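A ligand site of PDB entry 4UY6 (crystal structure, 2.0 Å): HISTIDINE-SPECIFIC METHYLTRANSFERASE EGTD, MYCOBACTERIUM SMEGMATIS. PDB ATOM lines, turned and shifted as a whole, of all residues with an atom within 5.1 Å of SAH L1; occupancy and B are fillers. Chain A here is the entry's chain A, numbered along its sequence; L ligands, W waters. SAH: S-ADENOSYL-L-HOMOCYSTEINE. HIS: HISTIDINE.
O of Asp 112 sits at hydrogen-bond distance from N of Gly 139, 3.0 Å away. OD2 of Asp 112 sits at hydrogen-bond distance from N of Gly 87, at 2.8 Å. The side-chain carboxylate (OD2) of Asp 112 lies within hydrogen-bond range of the backbone NH (N) of Ser 86. N of Asp 114 is in hydrogen-bond range of OD1 of Asp 112, at 3.0 Å. The side-chain carboxylate of Asp 140 lies within salt-bridge range of the side-chain amino group of Lys 35 (2.9 Å). The side-chain carboxylate (OD1) of Asp 140 lies within hydrogen-bond range of the backbone NH (N) of Glu 142 (3.0 Å). O of Phe 111 lies within hydrogen-bond range of N of Ser 86, 3.2 Å away. The backbone carbonyl oxygen of Glu 83 lies within hydrogen-bond range of the backbone NH of Phe 111.
Residues that only touch SAH L1: Tyr 38 (3.2 Å), Gly 139 (3.2 Å), Phe 46 (3.3 Å), Gly 160 (3.7 Å), Lys 35 (3.8 Å), Thr 162 (3.8 Å), Phe 111 (3.9 Å) and Leu 159 (3.9 Å). Within 4 Å of SAH L1: Lys 35, Tyr 38, Phe 46, Glu 83, Gly 85, Ser 86, Gly 87, Lys 91, Phe 111, Asp 112, Val 113, Gly 139, Asp 140, Phe 141, Leu 159, Gly 160 and Thr 162. Along chain A the residues within 4 Å of SAH L1 span positions 35 to 162. The nearest printed residue that does not touch SAH L1 is Asp 114 (4.4 Å).
Water W1 lies within hydrogen-bond range of O3' of SAH L1 (2.6 Å) and OG of Ser 43 (2.8 Å). Water W5 lies within hydrogen-bond range of an oxygen (O) of SAH L1 (2.7 Å) and the side-chain hydroxyl (OG1) of Thr 58 (2.8 Å). Water W2 lies within hydrogen-bond range of N of Leu 159, O of Leu 84, OE2 of Glu 83 and N of SAH L1.
O of Gly 85 is in hydrogen-bond range of N of SAH L1 (2.6 Å). NZ of Lys 91 is in salt-bridge range of OXT of SAH L1 (2.7 Å). An oxygen (O2') of SAH L1 sits at hydrogen-bond distance from the side-chain carboxylate (OD1) of Asp 112, 2.7 Å away. N of Phe 141 is in hydrogen-bond range of N1 of SAH L1, 2.9 Å away. The side-chain carboxylate of Asp 140 sits at hydrogen-bond distance from a nitrogen (N6) of SAH L1, 2.9 Å away. The backbone NH (N) of Val 113 lies within hydrogen-bond range of a nitrogen (N3) of SAH L1 (3.3 Å). The backbone NH (N) of Gly 87 sits close to an oxygen (O3') of SAH L1, 3.4 Å away. The backbone carbonyl oxygen (O) of Ser 86 sits at hydrogen-bond distance from a nitrogen (N) of SAH L1. The side-chain carboxylate (OE2) of Glu 83 is in salt-bridge range of a nitrogen (N) of SAH L1.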
ATOM      1  N   LYS A  35     -21.293 -22.308 -19.964  1.00  0.00           N
ATOM      2  CA  LYS A  35     -20.206 -23.011 -19.292  1.00  0.00           C
ATOM      3  C   LYS A  35     -20.627 -23.433 -17.882  1.00  0.00           C
ATOM      4  O   LYS A  35     -20.075 -24.378 -17.317  1.00  0.00           O
ATOM      5  CB  LYS A  35     -18.944 -22.149 -19.237  1.00  0.00           C
ATOM      6  CG  LYS A  35     -18.938 -21.043 -18.175  1.00  0.00           C
ATOM      7  CD  LYS A  35     -17.750 -20.091 -18.370  1.00  0.00           C
ATOM      8  CE  LYS A  35     -17.806 -19.483 -19.760  1.00  0.00           C
ATOM      9  NZ  LYS A  35     -17.002 -18.259 -19.902  1.00  0.00           N
ATOM     10  N   TYR A  38     -21.586 -27.004 -16.517  1.00  0.00           N
ATOM     11  CA  TYR A  38     -20.615 -28.083 -16.385  1.00  0.00           C
ATOM     12  C   TYR A  38     -19.802 -28.096 -15.082  1.00  0.00           C
ATOM     13  O   TYR A  38     -18.583 -27.927 -15.090  1.00  0.00           O
ATOM     14  CB  TYR A  38     -19.686 -28.033 -17.601  1.00  0.00           C
ATOM     15  CG  TYR A  38     -20.462 -28.125 -18.902  1.00  0.00           C
ATOM     16  CD1 TYR A  38     -20.850 -29.353 -19.402  1.00  0.00           C
ATOM     17  CD2 TYR A  38     -20.830 -26.973 -19.601  1.00  0.00           C
ATOM     18  CE1 TYR A  38     -21.564 -29.445 -20.581  1.00  0.00           C
ATOM     19  CE2 TYR A  38     -21.540 -27.059 -20.773  1.00  0.00           C
ATOM     20  CZ  TYR A  38     -21.910 -28.304 -21.253  1.00  0.00           C
ATOM     21  OH  TYR A  38     -22.623 -28.413 -22.418  1.00  0.00           O
ATOM     22  N   SER A  43     -21.614 -32.356 -15.987  1.00  0.00           N
ATOM     23  CA  SER A  43     -20.782 -33.102 -16.921  1.00  0.00           C
ATOM     24  C   SER A  43     -21.346 -34.501 -17.109  1.00  0.00           C
ATOM     25  O   SER A  43     -21.405 -35.018 -18.239  1.00  0.00           O
ATOM     26  CB  SER A  43     -19.328 -33.149 -16.425  1.00  0.00           C
ATOM     27  OG  SER A  43     -18.690 -31.908 -16.636  1.00  0.00           O
ATOM     28  N   PHE A  46     -24.652 -34.335 -19.189  1.00  0.00           N
ATOM     29  CA  PHE A  46     -24.403 -34.238 -20.626  1.00  0.00           C
ATOM     30  C   PHE A  46     -24.048 -35.614 -21.163  1.00  0.00           C
ATOM     31  O   PHE A  46     -24.444 -36.002 -22.269  1.00  0.00           O
ATOM     32  CB  PHE A  46     -23.292 -33.274 -20.976  1.00  0.00           C
ATOM     33  CG  PHE A  46     -22.916 -33.354 -22.428  1.00  0.00           C
ATOM     34  CD1 PHE A  46     -23.730 -32.781 -23.387  1.00  0.00           C
ATOM     35  CD2 PHE A  46     -21.792 -34.049 -22.835  1.00  0.00           C
ATOM     36  CE1 PHE A  46     -23.418 -32.871 -24.740  1.00  0.00           C
ATOM     37  CE2 PHE A  46     -21.458 -34.147 -24.178  1.00  0.00           C
ATOM     38  CZ  PHE A  46     -22.274 -33.561 -25.134  1.00  0.00           C
ATOM     39  N   THR A  50     -25.860 -37.775 -24.316  1.00  0.00           N
ATOM     40  CA  THR A  50     -25.224 -38.335 -25.519  1.00  0.00           C
ATOM     41  C   THR A  50     -25.785 -39.698 -25.883  1.00  0.00           C
ATOM     42  O   THR A  50     -25.581 -40.177 -27.000  1.00  0.00           O
ATOM     43  CB  THR A  50     -23.704 -38.498 -25.385  1.00  0.00           C
ATOM     44  OG1 THR A  50     -23.397 -39.515 -24.415  1.00  0.00           O
ATOM     45  CG2 THR A  50     -23.018 -37.171 -25.014  1.00  0.00           C
ATOM     46  N   THR A  58     -24.144 -37.075 -31.084  1.00  0.00           N
ATOM     47  CA  THR A  58     -22.944 -37.774 -30.603  1.00  0.00           C
ATOM     48  C   THR A  58     -22.668 -39.019 -31.453  1.00  0.00           C
ATOM     49  O   THR A  58     -21.555 -39.186 -31.940  1.00  0.00           O
ATOM     50  CB  THR A  58     -23.052 -38.155 -29.110  1.00  0.00           C
ATOM     51  OG1 THR A  58     -23.234 -36.976 -28.323  1.00  0.00           O
ATOM     52  CG2 THR A  58     -21.759 -38.849 -28.654  1.00  0.00           C
ATOM     53  N   GLU A  61     -21.612 -38.214 -35.136  1.00  0.00           N
ATOM     54  CA  GLU A  61     -20.220 -37.780 -35.206  1.00  0.00           C
ATOM     55  C   GLU A  61     -19.270 -38.949 -34.956  1.00  0.00           C
ATOM     56  O   GLU A  61     -18.243 -39.084 -35.623  1.00  0.00           O
ATOM     57  CB  GLU A  61     -19.957 -36.668 -34.185  1.00  0.00           C
ATOM     58  CG  GLU A  61     -18.626 -35.936 -34.353  1.00  0.00           C
ATOM     59  CD  GLU A  61     -18.506 -34.768 -33.375  1.00  0.00           C
ATOM     60  OE1 GLU A  61     -19.043 -34.878 -32.258  1.00  0.00           O
ATOM     61  OE2 GLU A  61     -17.883 -33.735 -33.740  1.00  0.00           O
ATOM     62  N   GLU A  83      -7.649 -31.155 -27.505  1.00  0.00           N
ATOM     63  CA  GLU A  83      -9.105 -31.192 -27.558  1.00  0.00           C
ATOM     64  C   GLU A  83      -9.772 -30.143 -26.702  1.00  0.00           C
ATOM     65  O   GLU A  83      -9.607 -30.107 -25.485  1.00  0.00           O
ATOM     66  CB  GLU A  83      -9.658 -32.555 -27.144  1.00  0.00           C
ATOM     67  CG  GLU A  83     -11.186 -32.544 -27.214  1.00  0.00           C
ATOM     68  CD  GLU A  83     -11.824 -33.896 -27.020  1.00  0.00           C
ATOM     69  OE1 GLU A  83     -11.195 -34.779 -26.379  1.00  0.00           O
ATOM     70  OE2 GLU A  83     -12.965 -34.087 -27.519  1.00  0.00           O
ATOM     71  N   LEU A  84     -10.543 -29.290 -27.357  1.00  0.00           N
ATOM     72  CA  LEU A  84     -11.239 -28.205 -26.688  1.00  0.00           C
ATOM     73  C   LEU A  84     -12.627 -28.642 -26.246  1.00  0.00           C
ATOM     74  O   LEU A  84     -13.362 -29.256 -27.007  1.00  0.00           O
ATOM     75  CB  LEU A  84     -11.339 -26.995 -27.605  1.00  0.00           C
ATOM     76  CG  LEU A  84      -9.984 -26.408 -28.045  1.00  0.00           C
ATOM     77  CD1 LEU A  84     -10.214 -25.264 -29.008  1.00  0.00           C
ATOM     78  CD2 LEU A  84      -9.192 -25.928 -26.830  1.00  0.00           C
ATOM     79  N   GLY A  85     -12.979 -28.307 -25.013  1.00  0.00           N
ATOM     80  CA  GLY A  85     -14.224 -28.763 -24.432  1.00  0.00           C
ATOM     81  C   GLY A  85     -14.226 -30.276 -24.464  1.00  0.00           C
ATOM     82  O   GLY A  85     -15.173 -30.918 -24.918  1.00  0.00           O
ATOM     83  N   SER A  86     -13.138 -30.841 -23.941  1.00  0.00           N
ATOM     84  CA  SER A  86     -12.854 -32.263 -24.103  1.00  0.00           C
ATOM     85  C   SER A  86     -13.845 -33.193 -23.418  1.00  0.00           C
ATOM     86  O   SER A  86     -14.142 -34.286 -23.940  1.00  0.00           O
ATOM     87  CB  SER A  86     -11.433 -32.568 -23.594  1.00  0.00           C
ATOM     88  OG  SER A  86     -11.294 -32.169 -22.249  1.00  0.00           O
ATOM     89  N   GLY A  87     -14.340 -32.773 -22.253  1.00  0.00           N
ATOM     90  CA  GLY A  87     -15.232 -33.601 -21.467  1.00  0.00           C
ATOM     91  C   GLY A  87     -14.552 -34.926 -21.154  1.00  0.00           C
ATOM     92  O   GLY A  87     -13.398 -34.973 -20.728  1.00  0.00           O
ATOM     93  N   LYS A  91     -15.080 -39.953 -27.789  1.00  0.00           N
ATOM     94  CA  LYS A  91     -14.909 -39.980 -29.249  1.00  0.00           C
ATOM     95  C   LYS A  91     -13.453 -39.788 -29.600  1.00  0.00           C
ATOM     96  O   LYS A  91     -12.967 -40.297 -30.613  1.00  0.00           O
ATOM     97  CB  LYS A  91     -15.746 -38.896 -29.926  1.00  0.00           C
ATOM     98  CG  LYS A  91     -17.247 -39.124 -29.875  1.00  0.00           C
ATOM     99  CD  LYS A  91     -17.974 -38.055 -30.681  1.00  0.00           C
ATOM    100  CE  LYS A  91     -18.641 -37.013 -29.792  1.00  0.00           C
ATOM    101  NZ  LYS A  91     -17.681 -36.122 -29.104  1.00  0.00           N
ATOM    102  N   PHE A 111      -8.555 -29.844 -22.841  1.00  0.00           N
ATOM    103  CA  PHE A 111      -8.786 -28.496 -22.401  1.00  0.00           C
ATOM    104  C   PHE A 111     -10.263 -28.409 -22.009  1.00  0.00           C
ATOM    105  O   PHE A 111     -11.126 -28.639 -22.848  1.00  0.00           O
ATOM    106  CB  PHE A 111      -8.426 -27.507 -23.529  1.00  0.00           C
ATOM    107  CG  PHE A 111      -8.568 -26.052 -23.158  1.00  0.00           C
ATOM    108  CD1 PHE A 111      -9.824 -25.483 -22.956  1.00  0.00           C
ATOM    109  CD2 PHE A 111      -7.436 -25.234 -23.038  1.00  0.00           C
ATOM    110  CE1 PHE A 111      -9.950 -24.133 -22.631  1.00  0.00           C
ATOM    111  CE2 PHE A 111      -7.558 -23.893 -22.708  1.00  0.00           C
ATOM    112  CZ  PHE A 111      -8.805 -23.339 -22.498  1.00  0.00           C
ATOM    113  N   ASP A 112     -10.548 -28.090 -20.741  1.00  0.00           N
ATOM    114  CA  ASP A 112     -11.925 -27.996 -20.279  1.00  0.00           C
ATOM    115  C   ASP A 112     -12.085 -27.019 -19.103  1.00  0.00           C
ATOM    116  O   ASP A 112     -11.116 -26.678 -18.416  1.00  0.00           O
ATOM    117  CB  ASP A 112     -12.448 -29.379 -19.864  1.00  0.00           C
ATOM    118  CG  ASP A 112     -13.936 -29.552 -20.109  1.00  0.00           C
ATOM    119  OD1 ASP A 112     -14.753 -28.980 -19.347  1.00  0.00           O
ATOM    120  OD2 ASP A 112     -14.314 -30.273 -21.066  1.00  0.00           O
ATOM    121  N   VAL A 113     -13.310 -26.545 -18.922  1.00  0.00           N
ATOM    122  CA  VAL A 113     -13.640 -25.642 -17.834  1.00  0.00           C
ATOM    123  C   VAL A 113     -13.754 -26.464 -16.554  1.00  0.00           C
ATOM    124  O   VAL A 113     -13.559 -25.964 -15.467  1.00  0.00           O
ATOM    125  CB  VAL A 113     -14.940 -24.837 -18.125  1.00  0.00           C
ATOM    126  CG1 VAL A 113     -16.174 -25.711 -17.901  1.00  0.00           C
ATOM    127  CG2 VAL A 113     -15.021 -23.628 -17.276  1.00  0.00           C
ATOM    128  N   ASP A 114     -14.019 -27.757 -16.693  1.00  0.00           N
ATOM    129  CA  ASP A 114     -14.233 -28.613 -15.530  1.00  0.00           C
ATOM    130  C   ASP A 114     -13.023 -29.478 -15.225  1.00  0.00           C
ATOM    131  O   ASP A 114     -12.722 -30.435 -15.953  1.00  0.00           O
ATOM    132  CB  ASP A 114     -15.476 -29.489 -15.754  1.00  0.00           C
ATOM    133  CG  ASP A 114     -15.738 -30.475 -14.610  1.00  0.00           C
ATOM    134  OD1 ASP A 114     -15.268 -30.256 -13.470  1.00  0.00           O
ATOM    135  OD2 ASP A 114     -16.439 -31.482 -14.851  1.00  0.00           O
ATOM    136  N   VAL A 117     -13.528 -33.443 -14.742  1.00  0.00           N
ATOM    137  CA  VAL A 117     -13.560 -34.170 -16.003  1.00  0.00           C
ATOM    138  C   VAL A 117     -12.157 -34.293 -16.595  1.00  0.00           C
ATOM    139  O   VAL A 117     -11.843 -35.297 -17.232  1.00  0.00           O
ATOM    140  CB  VAL A 117     -14.538 -33.499 -17.003  1.00  0.00           C
ATOM    141  CG1 VAL A 117     -13.829 -33.023 -18.256  1.00  0.00           C
ATOM    142  CG2 VAL A 117     -15.670 -34.457 -17.358  1.00  0.00           C
ATOM    143  N   GLY A 139      -9.278 -24.256 -18.317  1.00  0.00           N
ATOM    144  CA  GLY A 139      -9.508 -22.876 -18.702  1.00  0.00           C
ATOM    145  C   GLY A 139     -10.799 -22.696 -19.469  1.00  0.00           C
ATOM    146  O   GLY A 139     -11.574 -23.627 -19.651  1.00  0.00           O
ATOM    147  N   ASP A 140     -11.014 -21.459 -19.895  1.00  0.00           N
ATOM    148  CA  ASP A 140     -12.151 -21.041 -20.706  1.00  0.00           C
ATOM    149  C   ASP A 140     -11.693 -20.913 -22.153  1.00  0.00           C
ATOM    150  O   ASP A 140     -10.761 -20.164 -22.437  1.00  0.00           O
ATOM    151  CB  ASP A 140     -12.679 -19.705 -20.143  1.00  0.00           C
ATOM    152  CG  ASP A 140     -13.782 -19.094 -20.968  1.00  0.00           C
ATOM    153  OD1 ASP A 140     -14.238 -19.704 -21.965  1.00  0.00           O
ATOM    154  OD2 ASP A 140     -14.208 -17.996 -20.580  1.00  0.00           O
ATOM    155  N   PHE A 141     -12.307 -21.640 -23.093  1.00  0.00           N
ATOM    156  CA  PHE A 141     -11.761 -21.631 -24.455  1.00  0.00           C
ATOM    157  C   PHE A 141     -12.047 -20.315 -25.182  1.00  0.00           C
ATOM    158  O   PHE A 141     -11.628 -20.117 -26.313  1.00  0.00           O
ATOM    159  CB  PHE A 141     -12.240 -22.845 -25.303  1.00  0.00           C
ATOM    160  CG  PHE A 141     -13.756 -23.060 -25.356  1.00  0.00           C
ATOM    161  CD1 PHE A 141     -14.605 -22.068 -25.833  1.00  0.00           C
ATOM    162  CD2 PHE A 141     -14.302 -24.312 -25.055  1.00  0.00           C
ATOM    163  CE1 PHE A 141     -15.998 -22.281 -25.923  1.00  0.00           C
ATOM    164  CE2 PHE A 141     -15.686 -24.541 -25.137  1.00  0.00           C
ATOM    165  CZ  PHE A 141     -16.537 -23.514 -25.572  1.00  0.00           C
ATOM    166  N   GLU A 142     -12.747 -19.403 -24.518  1.00  0.00           N
ATOM    167  CA  GLU A 142     -12.948 -18.063 -25.082  1.00  0.00           C
ATOM    168  C   GLU A 142     -11.923 -17.077 -24.554  1.00  0.00           C
ATOM    169  O   GLU A 142     -11.925 -15.897 -24.944  1.00  0.00           O
ATOM    170  CB  GLU A 142     -14.342 -17.551 -24.759  1.00  0.00           C
ATOM    171  CG  GLU A 142     -15.452 -18.292 -25.454  1.00  0.00           C
ATOM    172  CD  GLU A 142     -16.791 -17.611 -25.263  1.00  0.00           C
ATOM    173  OE1 GLU A 142     -17.083 -16.665 -26.023  1.00  0.00           O
ATOM    174  OE2 GLU A 142     -17.546 -18.013 -24.347  1.00  0.00           O
ATOM    175  N   LEU A 159     -15.066 -30.910 -31.037  1.00  0.00           N
ATOM    176  CA  LEU A 159     -16.104 -31.822 -31.509  1.00  0.00           C
ATOM    177  C   LEU A 159     -17.463 -31.465 -30.942  1.00  0.00           C
ATOM    178  O   LEU A 159     -17.582 -30.535 -30.160  1.00  0.00           O
ATOM    179  CB  LEU A 159     -15.775 -33.259 -31.127  1.00  0.00           C
ATOM    180  CG  LEU A 159     -14.410 -33.738 -31.619  1.00  0.00           C
ATOM    181  CD1 LEU A 159     -14.169 -35.209 -31.248  1.00  0.00           C
ATOM    182  CD2 LEU A 159     -14.319 -33.576 -33.115  1.00  0.00           C
ATOM    183  N   GLY A 160     -18.475 -32.223 -31.347  1.00  0.00           N
ATOM    184  CA  GLY A 160     -19.786 -32.179 -30.721  1.00  0.00           C
ATOM    185  C   GLY A 160     -20.606 -30.944 -30.997  1.00  0.00           C
ATOM    186  O   GLY A 160     -21.620 -30.703 -30.314  1.00  0.00           O
ATOM    187  N   THR A 162     -19.944 -28.033 -30.243  1.00  0.00           N
ATOM    188  CA  THR A 162     -19.837 -27.070 -29.153  1.00  0.00           C
ATOM    189  C   THR A 162     -19.636 -25.669 -29.698  1.00  0.00           C
ATOM    190  O   THR A 162     -20.014 -24.686 -29.052  1.00  0.00           O
ATOM    191  CB  THR A 162     -18.685 -27.446 -28.187  1.00  0.00           C
ATOM    192  OG1 THR A 162     -18.846 -28.793 -27.780  1.00  0.00           O
ATOM    193  CG2 THR A 162     -18.683 -26.532 -26.928  1.00  0.00           C
HETATM  194  N   SAH L   1     -16.356 -32.866 -26.240  1.00  0.00           N
HETATM  195  CA  SAH L   1     -17.385 -33.680 -25.607  1.00  0.00           C
HETATM  196  CB  SAH L   1     -18.176 -32.870 -24.579  1.00  0.00           C
HETATM  197  CG  SAH L   1     -18.897 -31.697 -25.223  1.00  0.00           C
HETATM  198  SD  SAH L   1     -20.062 -30.852 -24.113  1.00  0.00           S
HETATM  199  C   SAH L   1     -18.325 -34.191 -26.690  1.00  0.00           C
HETATM  200  O   SAH L   1     -19.229 -34.979 -26.415  1.00  0.00           O
HETATM  201  OXT SAH L   1     -18.197 -33.818 -27.860  1.00  0.00           O
HETATM  202  C5' SAH L   1     -18.984 -29.385 -24.042  1.00  0.00           C
HETATM  203  C4' SAH L   1     -17.700 -29.577 -23.218  1.00  0.00           C
HETATM  204  O4' SAH L   1     -17.003 -28.331 -23.153  1.00  0.00           O
HETATM  205  C3' SAH L   1     -17.989 -29.958 -21.785  1.00  0.00           C
HETATM  206  O3' SAH L   1     -17.007 -30.871 -21.360  1.00  0.00           O
HETATM  207  C2' SAH L   1     -17.841 -28.646 -21.003  1.00  0.00           C
HETATM  208  O2' SAH L   1     -17.408 -28.899 -19.692  1.00  0.00           O
HETATM  209  C1' SAH L   1     -16.822 -27.875 -21.821  1.00  0.00           C
HETATM  210  N9  SAH L   1     -16.995 -26.405 -21.888  1.00  0.00           N
HETATM  211  C8  SAH L   1     -18.160 -25.671 -22.032  1.00  0.00           C
HETATM  212  N7  SAH L   1     -17.838 -24.352 -22.102  1.00  0.00           N
HETATM  213  C5  SAH L   1     -16.494 -24.245 -22.008  1.00  0.00           C
HETATM  214  C6  SAH L   1     -15.627 -23.149 -22.031  1.00  0.00           C
HETATM  215  N6  SAH L   1     -16.113 -21.917 -22.139  1.00  0.00           N
HETATM  216  N1  SAH L   1     -14.275 -23.363 -21.921  1.00  0.00           N
HETATM  217  C2  SAH L   1     -13.753 -24.626 -21.791  1.00  0.00           C
HETATM  218  N3  SAH L   1     -14.618 -25.698 -21.775  1.00  0.00           N
HETATM  219  C4  SAH L   1     -15.960 -25.513 -21.880  1.00  0.00           C
HETATM  220  N   HIS L   2     -22.823 -28.887 -27.007  1.00  0.00           N
HETATM  221  CA  HIS L   2     -24.128 -29.529 -26.845  1.00  0.00           C
HETATM  222  C   HIS L   2     -25.091 -29.069 -27.941  1.00  0.00           C
HETATM  223  O   HIS L   2     -25.848 -29.862 -28.508  1.00  0.00           O
HETATM  224  CB  HIS L   2     -24.702 -29.219 -25.459  1.00  0.00           C
HETATM  225  CG  HIS L   2     -26.103 -29.726 -25.249  1.00  0.00           C
HETATM  226  ND1 HIS L   2     -27.093 -28.952 -24.683  1.00  0.00           N
HETATM  227  CD2 HIS L   2     -26.672 -30.924 -25.538  1.00  0.00           C
HETATM  228  CE1 HIS L   2     -28.207 -29.647 -24.619  1.00  0.00           C
HETATM  229  NE2 HIS L   2     -27.987 -30.849 -25.136  1.00  0.00           N
HETATM  230  OXT HIS L   2     -25.118 -27.884 -28.294  1.00  0.00           O
HETATM  231  O   HOH W   1     -17.588 -32.171 -19.223  1.00  0.00           O
HETATM  232  O   HOH W   2     -14.132 -31.555 -28.558  1.00  0.00           O
HETATM  233  O   HOH W   3     -18.324 -35.571 -22.374  1.00  0.00           O
HETATM  234  O   HOH W   4     -16.655 -30.280 -27.414  1.00  0.00           O
HETATM  235  O   HOH W   5     -21.186 -35.030 -28.338  1.00  0.00           O
